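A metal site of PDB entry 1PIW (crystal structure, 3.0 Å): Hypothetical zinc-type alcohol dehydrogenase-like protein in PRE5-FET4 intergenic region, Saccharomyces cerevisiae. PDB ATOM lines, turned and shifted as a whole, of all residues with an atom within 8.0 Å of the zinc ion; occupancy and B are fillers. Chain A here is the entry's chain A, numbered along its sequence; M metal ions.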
ATOM      1  N   GLN A  96      11.636  32.353  -5.271  1.00  0.00           N
ATOM      2  CA  GLN A  96      12.285  31.927  -4.028  1.00  0.00           C
ATOM      3  C   GLN A  96      12.246  33.087  -3.035  1.00  0.00           C
ATOM      4  O   GLN A  96      12.241  34.252  -3.430  1.00  0.00           O
ATOM      5  CB  GLN A  96      13.721  31.457  -4.246  1.00  0.00           C
ATOM      6  CG  GLN A  96      14.213  30.598  -3.091  1.00  0.00           C
ATOM      7  CD  GLN A  96      15.576  29.998  -3.323  1.00  0.00           C
ATOM      8  OE1 GLN A  96      15.940  29.664  -4.443  1.00  0.00           O
ATOM      9  NE2 GLN A  96      16.340  29.832  -2.247  1.00  0.00           N
ATOM     10  N   PHE A  98      13.756  32.440   0.412  1.00  0.00           N
ATOM     11  CA  PHE A  98      14.634  32.058   1.509  1.00  0.00           C
ATOM     12  C   PHE A  98      15.574  30.897   1.185  1.00  0.00           C
ATOM     13  O   PHE A  98      15.257  30.030   0.361  1.00  0.00           O
ATOM     14  CB  PHE A  98      13.828  31.681   2.748  1.00  0.00           C
ATOM     15  CG  PHE A  98      14.682  31.333   3.915  1.00  0.00           C
ATOM     16  CD1 PHE A  98      15.327  32.335   4.641  1.00  0.00           C
ATOM     17  CD2 PHE A  98      14.899  30.005   4.263  1.00  0.00           C
ATOM     18  CE1 PHE A  98      16.188  32.031   5.682  1.00  0.00           C
ATOM     19  CE2 PHE A  98      15.756  29.682   5.315  1.00  0.00           C
ATOM     20  CZ  PHE A  98      16.406  30.703   6.031  1.00  0.00           C
ATOM     21  N   SER A  99      16.707  30.895   1.864  1.00  0.00           N
ATOM     22  CA  SER A  99      17.733  29.873   1.671  1.00  0.00           C
ATOM     23  C   SER A  99      18.625  29.873   2.917  1.00  0.00           C
ATOM     24  O   SER A  99      18.718  30.898   3.602  1.00  0.00           O
ATOM     25  CB  SER A  99      18.552  30.221   0.433  1.00  0.00           C
ATOM     26  OG  SER A  99      19.307  29.109   0.008  1.00  0.00           O
ATOM     27  N   CYS A 100      19.258  28.749   3.221  1.00  0.00           N
ATOM     28  CA  CYS A 100      20.102  28.689   4.420  1.00  0.00           C
ATOM     29  C   CYS A 100      21.276  29.643   4.280  1.00  0.00           C
ATOM     30  O   CYS A 100      21.887  30.015   5.274  1.00  0.00           O
ATOM     31  CB  CYS A 100      20.607  27.267   4.655  1.00  0.00           C
ATOM     32  SG  CYS A 100      22.074  26.851   3.735  1.00  0.00           S
ATOM     33  N   LEU A 101      21.575  30.009   3.044  1.00  0.00           N
ATOM     34  CA  LEU A 101      22.660  30.938   2.733  1.00  0.00           C
ATOM     35  C   LEU A 101      24.030  30.566   3.268  1.00  0.00           C
ATOM     36  O   LEU A 101      24.911  31.403   3.323  1.00  0.00           O
ATOM     37  CB  LEU A 101      22.298  32.339   3.216  1.00  0.00           C
ATOM     38  CG  LEU A 101      21.105  32.892   2.446  1.00  0.00           C
ATOM     39  CD1 LEU A 101      20.610  34.163   3.088  1.00  0.00           C
ATOM     40  CD2 LEU A 101      21.511  33.144   1.004  1.00  0.00           C
ATOM     41  N   GLU A 102      24.207  29.304   3.662  1.00  0.00           N
ATOM     42  CA  GLU A 102      25.497  28.865   4.190  1.00  0.00           C
ATOM     43  C   GLU A 102      26.041  27.579   3.582  1.00  0.00           C
ATOM     44  O   GLU A 102      27.254  27.364   3.580  1.00  0.00           O
ATOM     45  CB  GLU A 102      25.432  28.740   5.708  1.00  0.00           C
ATOM     46  CG  GLU A 102      25.798  30.032   6.406  1.00  0.00           C
ATOM     47  CD  GLU A 102      25.549  30.009   7.907  1.00  0.00           C
ATOM     48  OE1 GLU A 102      25.907  30.992   8.581  1.00  0.00           O
ATOM     49  OE2 GLU A 102      24.994  29.003   8.399  1.00  0.00           O
ATOM     50  N   CYS A 103      25.179  26.727   3.064  1.00  0.00           N
ATOM     51  CA  CYS A 103      25.668  25.497   2.464  1.00  0.00           C
ATOM     52  C   CYS A 103      26.423  25.801   1.173  1.00  0.00           C
ATOM     53  O   CYS A 103      26.333  26.906   0.630  1.00  0.00           O
ATOM     54  CB  CYS A 103      24.515  24.537   2.176  1.00  0.00           C
ATOM     55  SG  CYS A 103      23.411  25.060   0.871  1.00  0.00           S
ATOM     56  N   ASP A 104      27.187  24.823   0.692  1.00  0.00           N
ATOM     57  CA  ASP A 104      27.953  24.989  -0.531  1.00  0.00           C
ATOM     58  C   ASP A 104      27.071  25.488  -1.654  1.00  0.00           C
ATOM     59  O   ASP A 104      27.378  26.489  -2.298  1.00  0.00           O
ATOM     60  CB  ASP A 104      28.602  23.673  -0.946  1.00  0.00           C
ATOM     61  CG  ASP A 104      29.768  23.282  -0.047  1.00  0.00           C
ATOM     62  OD1 ASP A 104      30.303  22.170  -0.232  1.00  0.00           O
ATOM     63  OD2 ASP A 104      30.157  24.088   0.824  1.00  0.00           O
ATOM     64  N   ARG A 105      25.962  24.779  -1.885  1.00  0.00           N
ATOM     65  CA  ARG A 105      25.022  25.152  -2.933  1.00  0.00           C
ATOM     66  C   ARG A 105      24.657  26.626  -2.876  1.00  0.00           C
ATOM     67  O   ARG A 105      24.571  27.293  -3.897  1.00  0.00           O
ATOM     68  CB  ARG A 105      23.785  24.283  -2.829  1.00  0.00           C
ATOM     69  CG  ARG A 105      24.082  22.832  -3.130  1.00  0.00           C
ATOM     70  CD  ARG A 105      22.847  21.959  -3.091  1.00  0.00           C
ATOM     71  NE  ARG A 105      23.112  20.673  -3.725  1.00  0.00           N
ATOM     72  CZ  ARG A 105      22.190  19.739  -3.935  1.00  0.00           C
ATOM     73  NH1 ARG A 105      20.939  19.975  -3.562  1.00  0.00           N
ATOM     74  NH2 ARG A 105      22.514  18.599  -4.524  1.00  0.00           N
ATOM     75  N   CYS A 106      24.455  27.153  -1.674  1.00  0.00           N
ATOM     76  CA  CYS A 106      24.121  28.567  -1.541  1.00  0.00           C
ATOM     77  C   CYS A 106      25.283  29.465  -1.949  1.00  0.00           C
ATOM     78  O   CYS A 106      25.129  30.379  -2.763  1.00  0.00           O
ATOM     79  CB  CYS A 106      23.734  28.889  -0.114  1.00  0.00           C
ATOM     80  SG  CYS A 106      22.047  28.485   0.283  1.00  0.00           S
ATOM     81  N   LYS A 107      26.447  29.217  -1.359  1.00  0.00           N
ATOM     82  CA  LYS A 107      27.647  29.995  -1.596  1.00  0.00           C
ATOM     83  C   LYS A 107      28.145  29.848  -3.026  1.00  0.00           C
ATOM     84  O   LYS A 107      28.929  30.661  -3.525  1.00  0.00           O
ATOM     85  CB  LYS A 107      28.726  29.572  -0.594  1.00  0.00           C
ATOM     86  CG  LYS A 107      28.342  29.899   0.853  1.00  0.00           C
ATOM     87  CD  LYS A 107      29.315  29.364   1.897  1.00  0.00           C
ATOM     88  CE  LYS A 107      28.856  29.812   3.292  1.00  0.00           C
ATOM     89  NZ  LYS A 107      29.660  29.260   4.427  1.00  0.00           N
ATOM     90  N   ASN A 110      23.464  28.468  -5.994  1.00  0.00           N
ATOM     91  CA  ASN A 110      22.523  27.418  -6.329  1.00  0.00           C
ATOM     92  C   ASN A 110      21.465  27.308  -5.234  1.00  0.00           C
ATOM     93  O   ASN A 110      20.990  26.232  -4.919  1.00  0.00           O
ATOM     94  CB  ASN A 110      23.240  26.086  -6.517  1.00  0.00           C
ATOM     95  CG  ASN A 110      23.949  25.994  -7.863  1.00  0.00           C
ATOM     96  OD1 ASN A 110      23.334  26.192  -8.906  1.00  0.00           O
ATOM     97  ND2 ASN A 110      25.233  25.693  -7.835  1.00  0.00           N
ATOM     98  N   GLU A 111      21.100  28.463  -4.685  1.00  0.00           N
ATOM     99  CA  GLU A 111      20.123  28.523  -3.634  1.00  0.00           C
ATOM    100  C   GLU A 111      18.773  27.964  -4.027  1.00  0.00           C
ATOM    101  O   GLU A 111      17.948  27.679  -3.170  1.00  0.00           O
ATOM    102  CB  GLU A 111      19.971  29.945  -3.120  1.00  0.00           C
ATOM    103  CG  GLU A 111      19.785  30.992  -4.180  1.00  0.00           C
ATOM    104  CD  GLU A 111      21.083  31.642  -4.586  1.00  0.00           C
ATOM    105  OE1 GLU A 111      21.788  31.063  -5.441  1.00  0.00           O
ATOM    106  OE2 GLU A 111      21.402  32.714  -4.033  1.00  0.00           O
ATOM    107  N   PRO A 112      18.498  27.823  -5.327  1.00  0.00           N
ATOM    108  CA  PRO A 112      17.189  27.268  -5.647  1.00  0.00           C
ATOM    109  C   PRO A 112      17.174  25.797  -5.256  1.00  0.00           C
ATOM    110  O   PRO A 112      16.127  25.199  -5.068  1.00  0.00           O
ATOM    111  CB  PRO A 112      17.089  27.441  -7.152  1.00  0.00           C
ATOM    112  CG  PRO A 112      17.870  28.680  -7.391  1.00  0.00           C
ATOM    113  CD  PRO A 112      19.082  28.478  -6.516  1.00  0.00           C
ATOM    114  N   TYR A 113      18.374  25.227  -5.120  1.00  0.00           N
ATOM    115  CA  TYR A 113      18.540  23.827  -4.772  1.00  0.00           C
ATOM    116  C   TYR A 113      19.044  23.642  -3.341  1.00  0.00           C
ATOM    117  O   TYR A 113      19.632  22.613  -2.999  1.00  0.00           O
ATOM    118  CB  TYR A 113      19.530  23.174  -5.745  1.00  0.00           C
ATOM    119  CG  TYR A 113      19.212  23.484  -7.178  1.00  0.00           C
ATOM    120  CD1 TYR A 113      19.535  24.717  -7.736  1.00  0.00           C
ATOM    121  CD2 TYR A 113      18.490  22.581  -7.961  1.00  0.00           C
ATOM    122  CE1 TYR A 113      19.130  25.045  -9.034  1.00  0.00           C
ATOM    123  CE2 TYR A 113      18.084  22.903  -9.243  1.00  0.00           C
ATOM    124  CZ  TYR A 113      18.398  24.129  -9.779  1.00  0.00           C
ATOM    125  OH  TYR A 113      17.969  24.451 -11.043  1.00  0.00           O
ATOM    126  N   CYS A 114      18.816  24.650  -2.502  1.00  0.00           N
ATOM    127  CA  CYS A 114      19.234  24.556  -1.105  1.00  0.00           C
ATOM    128  C   CYS A 114      18.282  23.660  -0.360  1.00  0.00           C
ATOM    129  O   CYS A 114      17.095  23.585  -0.673  1.00  0.00           O
ATOM    130  CB  CYS A 114      19.270  25.928  -0.452  1.00  0.00           C
ATOM    131  SG  CYS A 114      19.382  25.861   1.356  1.00  0.00           S
ATOM    132  N   THR A 115      18.802  22.978   0.644  1.00  0.00           N
ATOM    133  CA  THR A 115      18.011  22.073   1.455  1.00  0.00           C
ATOM    134  C   THR A 115      16.879  22.806   2.167  1.00  0.00           C
ATOM    135  O   THR A 115      15.773  22.281   2.308  1.00  0.00           O
ATOM    136  CB  THR A 115      18.904  21.406   2.527  1.00  0.00           C
ATOM    137  OG1 THR A 115      20.025  20.785   1.899  1.00  0.00           O
ATOM    138  CG2 THR A 115      18.117  20.375   3.329  1.00  0.00           C
ATOM    139  N   LYS A 116      17.176  24.011   2.637  1.00  0.00           N
ATOM    140  CA  LYS A 116      16.213  24.831   3.375  1.00  0.00           C
ATOM    141  C   LYS A 116      15.452  25.811   2.478  1.00  0.00           C
ATOM    142  O   LYS A 116      15.030  26.889   2.917  1.00  0.00           O
ATOM    143  CB  LYS A 116      16.974  25.602   4.449  1.00  0.00           C
ATOM    144  CG  LYS A 116      18.123  24.819   5.077  1.00  0.00           C
ATOM    145  CD  LYS A 116      17.717  24.106   6.375  1.00  0.00           C
ATOM    146  CE  LYS A 116      16.801  22.920   6.110  1.00  0.00           C
ATOM    147  NZ  LYS A 116      16.293  22.299   7.386  1.00  0.00           N
ATOM    148  N   PHE A 117      15.291  25.439   1.217  1.00  0.00           N
ATOM    149  CA  PHE A 117      14.605  26.252   0.223  1.00  0.00           C
ATOM    150  C   PHE A 117      13.194  26.608   0.644  1.00  0.00           C
ATOM    151  O   PHE A 117      12.504  25.797   1.255  1.00  0.00           O
ATOM    152  CB  PHE A 117      14.556  25.473  -1.116  1.00  0.00           C
ATOM    153  CG  PHE A 117      13.637  26.085  -2.137  1.00  0.00           C
ATOM    154  CD1 PHE A 117      14.117  26.968  -3.085  1.00  0.00           C
ATOM    155  CD2 PHE A 117      12.274  25.758  -2.163  1.00  0.00           C
ATOM    156  CE1 PHE A 117      13.271  27.503  -4.041  1.00  0.00           C
ATOM    157  CE2 PHE A 117      11.434  26.296  -3.111  1.00  0.00           C
ATOM    158  CZ  PHE A 117      11.928  27.172  -4.055  1.00  0.00           C
HETATM  159 ZN    ZN M   1      21.741  26.476   1.499  1.00  0.00          ZN
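Ser 99 touches the zinc ion. Leu 101 touches the zinc ion (N to ZN, 3.9 Å). Six residues have an atom within 4 Å of the zinc ion: Ser 99, Cys 100, Leu 101, Cys 103, Cys 106 and Cys 114.
The backbone NH of Lys 116 sits close to the side-chain sulfur of Cys 114, at 3.2 Å. The backbone NH (N) of Arg 105 sits close to the side-chain sulfur (SG) of Cys 103, at 3.8 Å. The side-chain sulfur (SG) of Cys 114 lies close to the side-chain hydroxyl (OG) of Ser 99 (3.5 Å). The side-chain sulfur of Cys 106 lies close to the side-chain hydroxyl of Ser 99. SG of Cys 106 sits close to N of Leu 101, 3.2 Å away. N of Glu 102 sits close to SG of Cys 100 (3.3 Å).
SG of Cys 103 is bound to the zinc ion. The zinc ion is bound by the side-chain sulfur (SG) of Cys 100 (2.3 Å). The zinc ion is bound by SG of Cys 106, at 2.4 Å. The side-chain sulfur (SG) of Cys 114 is bound to the zinc ion.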
